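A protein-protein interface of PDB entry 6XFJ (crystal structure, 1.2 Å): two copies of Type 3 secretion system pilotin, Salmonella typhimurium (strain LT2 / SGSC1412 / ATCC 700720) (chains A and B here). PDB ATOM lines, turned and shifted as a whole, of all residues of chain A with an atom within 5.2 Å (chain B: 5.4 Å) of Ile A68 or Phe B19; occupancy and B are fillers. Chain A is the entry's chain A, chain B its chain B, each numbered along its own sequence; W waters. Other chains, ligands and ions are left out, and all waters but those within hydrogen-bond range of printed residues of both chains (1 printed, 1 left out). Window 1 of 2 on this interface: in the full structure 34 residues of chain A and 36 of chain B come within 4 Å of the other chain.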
ATOM      1  N   THR A  26      -6.003 -23.287  -4.229  1.00  0.00           N
ATOM      2  CA  THR A  26      -6.138 -21.908  -4.734  1.00  0.00           C
ATOM      3  C   THR A  26      -7.538 -21.353  -4.475  1.00  0.00           C
ATOM      4  O   THR A  26      -7.654 -20.176  -4.035  1.00  0.00           O
ATOM      5  CB  THR A  26      -5.766 -21.877  -6.222  1.00  0.00           C
ATOM      6  OG1 THR A  26      -4.359 -22.126  -6.319  1.00  0.00           O
ATOM      7  CG2 THR A  26      -6.047 -20.560  -6.911  1.00  0.00           C
ATOM      8  N   GLN A  29      -7.782 -20.531  -0.829  1.00  0.00           N
ATOM      9  CA  GLN A  29      -6.985 -19.327  -0.500  1.00  0.00           C
ATOM     10  C   GLN A  29      -7.710 -18.060  -0.949  1.00  0.00           C
ATOM     11  O   GLN A  29      -7.726 -17.083  -0.191  1.00  0.00           O
ATOM     12  CB  GLN A  29      -5.620 -19.415  -1.168  1.00  0.00           C
ATOM     13  CG  GLN A  29      -4.695 -20.377  -0.451  1.00  0.00           C
ATOM     14  CD  GLN A  29      -3.430 -20.628  -1.227  1.00  0.00           C
ATOM     15  OE1 GLN A  29      -3.129 -19.947  -2.231  1.00  0.00           O
ATOM     16  NE2 GLN A  29      -2.650 -21.595  -0.804  1.00  0.00           N
ATOM     17  N   ALA A  30      -8.340 -18.104  -2.099  1.00  0.00           N
ATOM     18  CA  ALA A  30      -9.020 -16.894  -2.601  1.00  0.00           C
ATOM     19  C   ALA A  30     -10.209 -16.604  -1.693  1.00  0.00           C
ATOM     20  O   ALA A  30     -10.446 -15.464  -1.288  1.00  0.00           O
ATOM     21  CB  ALA A  30      -9.439 -17.053  -4.043  1.00  0.00           C
ATOM     22  N   PHE A  54      -3.891  -6.943  -9.031  1.00  0.00           N
ATOM     23  CA  PHE A  54      -3.545  -8.370  -8.955  1.00  0.00           C
ATOM     24  C   PHE A  54      -2.899  -8.810 -10.276  1.00  0.00           C
ATOM     25  O   PHE A  54      -1.944  -9.503 -10.260  1.00  0.00           O
ATOM     26  CB  PHE A  54      -4.834  -9.113  -8.596  1.00  0.00           C
ATOM     27  CG  PHE A  54      -4.815 -10.618  -8.562  1.00  0.00           C
ATOM     28  CD1 PHE A  54      -3.935 -11.300  -7.739  1.00  0.00           C
ATOM     29  CD2 PHE A  54      -5.696 -11.315  -9.368  1.00  0.00           C
ATOM     30  CE1 PHE A  54      -4.013 -12.691  -7.653  1.00  0.00           C
ATOM     31  CE2 PHE A  54      -5.782 -12.702  -9.251  1.00  0.00           C
ATOM     32  CZ  PHE A  54      -4.886 -13.360  -8.467  1.00  0.00           C
ATOM     33  N   LEU A  58       0.928 -10.333 -10.757  1.00  0.00           N
ATOM     34  CA  LEU A  58       1.198 -11.666 -11.319  1.00  0.00           C
ATOM     35  C   LEU A  58       2.170 -11.568 -12.497  1.00  0.00           C
ATOM     36  O   LEU A  58       2.738 -12.600 -12.884  1.00  0.00           O
ATOM     37  CB  LEU A  58      -0.094 -12.367 -11.744  1.00  0.00           C
ATOM     38  CG  LEU A  58      -0.979 -12.757 -10.552  1.00  0.00           C
ATOM     39  CD1 LEU A  58      -2.248 -13.356 -11.115  1.00  0.00           C
ATOM     40  CD2 LEU A  58      -0.236 -13.714  -9.639  1.00  0.00           C
ATOM     41  N   LEU A  66       4.769 -17.161  -5.821  1.00  0.00           N
ATOM     42  CA  LEU A  66       3.818 -16.846  -4.748  1.00  0.00           C
ATOM     43  C   LEU A  66       2.442 -17.426  -5.037  1.00  0.00           C
ATOM     44  O   LEU A  66       2.010 -17.748  -6.120  1.00  0.00           O
ATOM     45  CB  LEU A  66       3.705 -15.324  -4.596  1.00  0.00           C
ATOM     46  CG  LEU A  66       5.034 -14.614  -4.316  1.00  0.00           C
ATOM     47  CD1 LEU A  66       4.760 -13.154  -4.022  1.00  0.00           C
ATOM     48  CD2 LEU A  66       5.788 -15.267  -3.150  1.00  0.00           C
ATOM     49  N   SER A  67       1.725 -17.680  -3.919  1.00  0.00           N
ATOM     50  CA  SER A  67       0.373 -18.281  -3.966  1.00  0.00           C
ATOM     51  C   SER A  67      -0.643 -17.235  -4.334  1.00  0.00           C
ATOM     52  O   SER A  67      -0.376 -16.001  -4.318  1.00  0.00           O
ATOM     53  CB  SER A  67      -0.046 -18.898  -2.654  1.00  0.00           C
ATOM     54  OG  SER A  67      -0.188 -17.837  -1.720  1.00  0.00           O
ATOM     55  N   ILE A  68      -1.880 -17.640  -4.616  1.00  0.00           N
ATOM     56  CA  ILE A  68      -2.933 -16.661  -4.883  1.00  0.00           C
ATOM     57  C   ILE A  68      -3.190 -15.809  -3.632  1.00  0.00           C
ATOM     58  O   ILE A  68      -3.469 -14.644  -3.713  1.00  0.00           O
ATOM     59  CB  ILE A  68      -4.206 -17.300  -5.425  1.00  0.00           C
ATOM     60  CG1 ILE A  68      -5.076 -16.245  -6.065  1.00  0.00           C
ATOM     61  CG2 ILE A  68      -4.988 -18.051  -4.342  1.00  0.00           C
ATOM     62  CD1 ILE A  68      -6.290 -16.731  -6.799  1.00  0.00           C
ATOM     63  N   TYR A  69      -3.092 -16.406  -2.427  1.00  0.00           N
ATOM     64  CA  TYR A  69      -3.276 -15.594  -1.215  1.00  0.00           C
ATOM     65  C   TYR A  69      -2.235 -14.500  -1.123  1.00  0.00           C
ATOM     66  O   TYR A  69      -2.542 -13.387  -0.820  1.00  0.00           O
ATOM     67  CB  TYR A  69      -3.297 -16.532   0.003  1.00  0.00           C
ATOM     68  CG  TYR A  69      -3.527 -15.800   1.286  1.00  0.00           C
ATOM     69  CD1 TYR A  69      -4.820 -15.564   1.729  1.00  0.00           C
ATOM     70  CD2 TYR A  69      -2.501 -15.424   2.117  1.00  0.00           C
ATOM     71  CE1 TYR A  69      -5.093 -14.862   2.892  1.00  0.00           C
ATOM     72  CE2 TYR A  69      -2.742 -14.734   3.298  1.00  0.00           C
ATOM     73  CZ  TYR A  69      -4.038 -14.464   3.694  1.00  0.00           C
ATOM     74  OH  TYR A  69      -4.279 -13.804   4.880  1.00  0.00           O
ATOM     75  N   GLN A  70      -0.995 -14.911  -1.308  1.00  0.00           N
ATOM     76  CA  GLN A  70       0.137 -13.951  -1.127  1.00  0.00           C
ATOM     77  C   GLN A  70       0.077 -12.839  -2.195  1.00  0.00           C
ATOM     78  O   GLN A  70       0.339 -11.666  -1.886  1.00  0.00           O
ATOM     79  CB  GLN A  70       1.480 -14.653  -1.243  1.00  0.00           C
ATOM     80  CG  GLN A  70       1.709 -15.654  -0.100  1.00  0.00           C
ATOM     81  CD  GLN A  70       2.659 -16.781  -0.437  1.00  0.00           C
ATOM     82  OE1 GLN A  70       3.139 -16.956  -1.556  1.00  0.00           O
ATOM     83  NE2 GLN A  70       2.887 -17.651   0.550  1.00  0.00           N
ATOM     84  N   THR A  71      -0.395 -13.181  -3.387  1.00  0.00           N
ATOM     85  CA  THR A  71      -0.443 -12.152  -4.469  1.00  0.00           C
ATOM     86  C   THR A  71      -1.678 -11.257  -4.319  1.00  0.00           C
ATOM     87  O   THR A  71      -1.597 -10.057  -4.604  1.00  0.00           O
ATOM     88  CB  THR A  71      -0.296 -12.815  -5.829  1.00  0.00           C
ATOM     89  OG1 THR A  71      -1.238 -13.842  -6.048  1.00  0.00           O
ATOM     90  CG2 THR A  71       1.076 -13.394  -6.071  1.00  0.00           C
ATOM     91  N   LEU A  72      -2.816 -11.805  -3.855  1.00  0.00           N
ATOM     92  CA  LEU A  72      -3.971 -10.935  -3.494  1.00  0.00           C
ATOM     93  C   LEU A  72      -3.563 -10.018  -2.355  1.00  0.00           C
ATOM     94  O   LEU A  72      -3.920  -8.839  -2.416  1.00  0.00           O
ATOM     95  CB  LEU A  72      -5.195 -11.787  -3.108  1.00  0.00           C
ATOM     96  CG  LEU A  72      -5.858 -12.458  -4.301  1.00  0.00           C
ATOM     97  CD1 LEU A  72      -6.783 -13.558  -3.797  1.00  0.00           C
ATOM     98  CD2 LEU A  72      -6.618 -11.463  -5.162  1.00  0.00           C
ATOM     99  N   LEU A  73      -2.841 -10.485  -1.327  1.00  0.00           N
ATOM    100  CA  LEU A  73      -2.417  -9.599  -0.228  1.00  0.00           C
ATOM    101  C   LEU A  73      -1.511  -8.502  -0.807  1.00  0.00           C
ATOM    102  O   LEU A  73      -1.648  -7.344  -0.428  1.00  0.00           O
ATOM    103  CB  LEU A  73      -1.647 -10.386   0.848  1.00  0.00           C
ATOM    104  CG  LEU A  73      -2.303 -11.240   1.904  1.00  0.00           C
ATOM    105  CD1 LEU A  73      -1.246 -11.711   2.858  1.00  0.00           C
ATOM    106  CD2 LEU A  73      -3.321 -10.464   2.654  1.00  0.00           C
ATOM    107  N   ILE B  14     -13.503 -15.484  -9.918  1.00  0.00           N
ATOM    108  CA  ILE B  14     -12.831 -14.576 -10.873  1.00  0.00           C
ATOM    109  C   ILE B  14     -11.312 -14.643 -10.611  1.00  0.00           C
ATOM    110  O   ILE B  14     -10.525 -14.786 -11.567  1.00  0.00           O
ATOM    111  CB  ILE B  14     -13.379 -13.149 -10.738  1.00  0.00           C
ATOM    112  CG1 ILE B  14     -14.801 -13.083 -11.292  1.00  0.00           C
ATOM    113  CG2 ILE B  14     -12.482 -12.143 -11.424  1.00  0.00           C
ATOM    114  CD1 ILE B  14     -14.927 -12.994 -12.797  1.00  0.00           C
ATOM    115  N   SER B  15     -10.889 -14.492  -9.363  1.00  0.00           N
ATOM    116  CA  SER B  15      -9.452 -14.360  -9.055  1.00  0.00           C
ATOM    117  C   SER B  15      -8.751 -15.686  -9.345  1.00  0.00           C
ATOM    118  O   SER B  15      -7.638 -15.690  -9.887  1.00  0.00           O
ATOM    119  CB  SER B  15      -9.215 -13.830  -7.664  1.00  0.00           C
ATOM    120  OG  SER B  15      -9.732 -14.709  -6.684  1.00  0.00           O
ATOM    121  N   SER B  16      -9.373 -16.812  -8.975  1.00  0.00           N
ATOM    122  CA  SER B  16      -8.745 -18.131  -9.188  1.00  0.00           C
ATOM    123  C   SER B  16      -8.623 -18.374 -10.694  1.00  0.00           C
ATOM    124  O   SER B  16      -7.631 -18.974 -11.120  1.00  0.00           O
ATOM    125  CB  SER B  16      -9.465 -19.270  -8.516  1.00  0.00           C
ATOM    126  OG  SER B  16      -9.513 -19.131  -7.090  1.00  0.00           O
ATOM    127  N   SER B  17      -9.593 -17.953 -11.493  1.00  0.00           N
ATOM    128  CA  SER B  17      -9.504 -18.157 -12.964  1.00  0.00           C
ATOM    129  C   SER B  17      -8.346 -17.331 -13.542  1.00  0.00           C
ATOM    130  O   SER B  17      -7.637 -17.824 -14.344  1.00  0.00           O
ATOM    131  CB  SER B  17     -10.830 -17.819 -13.607  1.00  0.00           C
ATOM    132  OG  SER B  17     -10.729 -17.927 -15.012  1.00  0.00           O
ATOM    133  N   ILE B  18      -8.168 -16.116 -13.044  1.00  0.00           N
ATOM    134  CA  ILE B  18      -6.997 -15.304 -13.467  1.00  0.00           C
ATOM    135  C   ILE B  18      -5.713 -16.055 -13.098  1.00  0.00           C
ATOM    136  O   ILE B  18      -4.834 -16.255 -13.941  1.00  0.00           O
ATOM    137  CB  ILE B  18      -7.026 -13.914 -12.823  1.00  0.00           C
ATOM    138  CG1 ILE B  18      -8.180 -13.057 -13.357  1.00  0.00           C
ATOM    139  CG2 ILE B  18      -5.671 -13.228 -13.068  1.00  0.00           C
ATOM    140  CD1 ILE B  18      -8.447 -11.843 -12.548  1.00  0.00           C
ATOM    141  N   PHE B  19      -5.577 -16.517 -11.851  1.00  0.00           N
ATOM    142  CA  PHE B  19      -4.317 -17.091 -11.367  1.00  0.00           C
ATOM    143  C   PHE B  19      -4.041 -18.409 -12.104  1.00  0.00           C
ATOM    144  O   PHE B  19      -2.903 -18.732 -12.464  1.00  0.00           O
ATOM    145  CB  PHE B  19      -4.472 -17.352  -9.868  1.00  0.00           C
ATOM    146  CG  PHE B  19      -3.219 -17.810  -9.186  1.00  0.00           C
ATOM    147  CD1 PHE B  19      -2.986 -19.164  -8.937  1.00  0.00           C
ATOM    148  CD2 PHE B  19      -2.285 -16.896  -8.703  1.00  0.00           C
ATOM    149  CE1 PHE B  19      -1.874 -19.566  -8.240  1.00  0.00           C
ATOM    150  CE2 PHE B  19      -1.157 -17.312  -8.020  1.00  0.00           C
ATOM    151  CZ  PHE B  19      -0.932 -18.659  -7.807  1.00  0.00           C
ATOM    152  N   CYS B  20      -5.069 -19.267 -12.188  1.00  0.00           N
ATOM    153  CA  CYS B  20      -4.929 -20.670 -12.584  1.00  0.00           C
ATOM    154  C   CYS B  20      -5.247 -20.906 -14.069  1.00  0.00           C
ATOM    155  O   CYS B  20      -4.652 -21.872 -14.625  1.00  0.00           O
ATOM    156  CB  CYS B  20      -5.828 -21.511 -11.688  1.00  0.00           C
ATOM    157  SG  CYS B  20      -6.346 -23.150 -12.302  1.00  0.00           S
ATOM    158  N   GLU B  21      -6.200 -20.217 -14.640  1.00  0.00           N
ATOM    159  CA  GLU B  21      -6.639 -20.506 -16.017  1.00  0.00           C
ATOM    160  C   GLU B  21      -5.990 -19.522 -17.025  1.00  0.00           C
ATOM    161  O   GLU B  21      -5.677 -19.945 -18.123  1.00  0.00           O
ATOM    162  CB  GLU B  21      -8.157 -20.487 -16.110  1.00  0.00           C
ATOM    163  CG  GLU B  21      -8.827 -21.562 -15.248  1.00  0.00           C
ATOM    164  CD  GLU B  21     -10.340 -21.575 -15.053  1.00  0.00           C
ATOM    165  OE1 GLU B  21     -10.866 -22.648 -14.594  1.00  0.00           O
ATOM    166  OE2 GLU B  21     -11.007 -20.574 -15.349  1.00  0.00           O
ATOM    167  N   LYS B  22      -5.731 -18.279 -16.630  1.00  0.00           N
ATOM    168  CA  LYS B  22      -5.137 -17.246 -17.521  1.00  0.00           C
ATOM    169  C   LYS B  22      -3.607 -17.271 -17.386  1.00  0.00           C
ATOM    170  O   LYS B  22      -2.880 -17.505 -18.379  1.00  0.00           O
ATOM    171  CB  LYS B  22      -5.693 -15.872 -17.133  1.00  0.00           C
ATOM    172  N   TYR B  23      -3.108 -17.028 -16.182  1.00  0.00           N
ATOM    173  CA  TYR B  23      -1.665 -17.020 -15.894  1.00  0.00           C
ATOM    174  C   TYR B  23      -1.056 -18.406 -15.821  1.00  0.00           C
ATOM    175  O   TYR B  23       0.131 -18.604 -16.012  1.00  0.00           O
ATOM    176  CB  TYR B  23      -1.302 -16.184 -14.691  1.00  0.00           C
ATOM    177  CG  TYR B  23      -1.402 -14.700 -14.889  1.00  0.00           C
ATOM    178  CD1 TYR B  23      -2.587 -14.036 -14.923  1.00  0.00           C
ATOM    179  CD2 TYR B  23      -0.250 -13.985 -15.082  1.00  0.00           C
ATOM    180  CE1 TYR B  23      -2.660 -12.664 -15.094  1.00  0.00           C
ATOM    181  CE2 TYR B  23      -0.299 -12.616 -15.273  1.00  0.00           C
ATOM    182  CZ  TYR B  23      -1.502 -11.948 -15.273  1.00  0.00           C
ATOM    183  OH  TYR B  23      -1.588 -10.566 -15.421  1.00  0.00           O
ATOM    184  N   LYS B  24      -1.852 -19.376 -15.364  1.00  0.00           N
ATOM    185  CA  LYS B  24      -1.389 -20.778 -15.150  1.00  0.00           C
ATOM    186  C   LYS B  24      -0.202 -20.811 -14.177  1.00  0.00           C
ATOM    187  O   LYS B  24       0.760 -21.555 -14.397  1.00  0.00           O
ATOM    188  CB  LYS B  24      -1.139 -21.493 -16.477  1.00  0.00           C
ATOM    189  CG  LYS B  24      -2.429 -21.605 -17.294  1.00  0.00           C
ATOM    190  CD  LYS B  24      -2.347 -22.515 -18.466  1.00  0.00           C
ATOM    191  CE  LYS B  24      -3.618 -22.525 -19.274  1.00  0.00           C
ATOM    192  NZ  LYS B  24      -3.580 -23.600 -20.290  1.00  0.00           N
ATOM    193  N   GLN B  25      -0.293 -20.038 -13.096  1.00  0.00           N
ATOM    194  CA  GLN B  25       0.823 -19.934 -12.143  1.00  0.00           C
ATOM    195  C   GLN B  25       1.149 -21.287 -11.501  1.00  0.00           C
ATOM    196  O   GLN B  25       2.334 -21.567 -11.277  1.00  0.00           O
ATOM    197  CB  GLN B  25       0.572 -18.881 -11.077  1.00  0.00           C
ATOM    198  CG  GLN B  25       0.507 -17.481 -11.546  1.00  0.00           C
ATOM    199  CD  GLN B  25       1.797 -17.044 -12.206  1.00  0.00           C
ATOM    200  OE1 GLN B  25       1.839 -16.870 -13.408  1.00  0.00           O
ATOM    201  NE2 GLN B  25       2.807 -16.859 -11.409  1.00  0.00           N
ATOM    202  N   THR B  26       0.147 -22.073 -11.089  1.00  0.00           N
ATOM    203  CA  THR B  26       0.423 -23.346 -10.396  1.00  0.00           C
ATOM    204  C   THR B  26       1.249 -24.285 -11.292  1.00  0.00           C
ATOM    205  O   THR B  26       2.234 -24.834 -10.842  1.00  0.00           O
ATOM    206  CB  THR B  26      -0.890 -23.944  -9.893  1.00  0.00           C
ATOM    207  OG1 THR B  26      -1.329 -23.033  -8.879  1.00  0.00           O
ATOM    208  CG2 THR B  26      -0.743 -25.332  -9.302  1.00  0.00           C
ATOM    209  N   GLN B  29       4.798 -23.045 -11.665  1.00  0.00           N
ATOM    210  CA  GLN B  29       5.569 -23.226 -10.419  1.00  0.00           C
ATOM    211  C   GLN B  29       5.984 -24.693 -10.272  1.00  0.00           C
ATOM    212  O   GLN B  29       7.123 -24.989  -9.881  1.00  0.00           O
ATOM    213  CB  GLN B  29       4.701 -22.815  -9.246  1.00  0.00           C
ATOM    214  CG  GLN B  29       4.623 -21.300  -9.100  1.00  0.00           C
ATOM    215  CD  GLN B  29       3.628 -20.864  -8.055  1.00  0.00           C
ATOM    216  OE1 GLN B  29       3.165 -21.682  -7.274  1.00  0.00           O
ATOM    217  NE2 GLN B  29       3.279 -19.588  -7.989  1.00  0.00           N
HETATM  218  O   HOH W   1       2.394 -16.355  -8.570  1.00  0.00           O
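Positions printed for both chains: 26 and 29.
N of Tyr A69 sits close to OG of Ser A67 (3.3 Å). The side-chain amide oxygen (OE1) of Gln A70 sits at hydrogen-bond distance from the backbone NH (N) of Ser A67 (2.8 Å). OG1 of Thr A71 sits at hydrogen-bond distance from O of Ser A67. OG1 of Thr A71 sits at hydrogen-bond distance from O of Ile A68, at 3.3 Å. The backbone NH of Gln B25 sits at hydrogen-bond distance from the backbone carbonyl oxygen of Phe B19, 3.0 Å away. O of Phe B19 is in hydrogen-bond range of N of Lys B24.
Of the printed residues of chain B, Ile A68 touches Ser B15 (3.5 Å), Ser B16 (3.7 Å) and Phe B19 (3.5 Å). Of the printed residues of chain A, Phe B19 touches Thr A26 (3.9 Å), Leu A58 (3.9 Å), Leu A66 (3.5 Å), Ser A67 (3.7 Å), Ile A68 (3.5 Å) and Thr A71 (3.99 Å). Of the printed residues of chain A, Ile B18 touches Phe A54 (3.9 Å) and Leu A58 (3.9 Å). Of the printed residues of chain B, Phe A54 touches Ser B15 (3.6 Å) and Ile B18 (3.9 Å). Of the printed residues of chain B, Thr A26 touches Ser B16 (3.7 Å) and Phe B19 (3.9 Å). Lys B22 touches none of the printed residues of chain A. The nearest printed residue of chain B that does not touch Ile A68 is Ser B17 (5.9 Å). The nearest printed residue of chain A that does not touch Phe B19 is Phe A54 (4.3 Å).
O of Thr A26 touches OG of Ser B16 (3.7 Å). Ser B16 touches Ala A30. CE2 of Phe A54 touches O of Ser B15, at 3.6 Å. CE2 of Phe A54 touches CG2 of Ile B18 (3.9 Å). Phe B19 touches Leu A58. Leu A58 touches Tyr B23 (CB to CE2, 3.5 Å). Ser A67 touches Phe B19 (C to CE2, 3.7 Å). Ile A68 touches Ser B15. Ile A68 touches Ser B16. Thr A71 touches Phe B19.
Water W1 lies within hydrogen-bond range of the backbone carbonyl oxygen of Leu A66 (2.8 Å), the side-chain amide nitrogen of Gln B25 (2.9 Å) and the side-chain amide nitrogen of Gln B29 (3.4 Å).
O of Leu A66 sits at hydrogen-bond distance from NE2 of Gln B29.
Of the 14 printed residues of chain B, 6 touch a printed residue of chain A. Hydrophobic or aromatic side chains of chain B within 4 Å of the printed part of chain A: Ile B18, Phe B19 and Tyr B23. Among the printed residues, 16 pairs touch across the chains.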
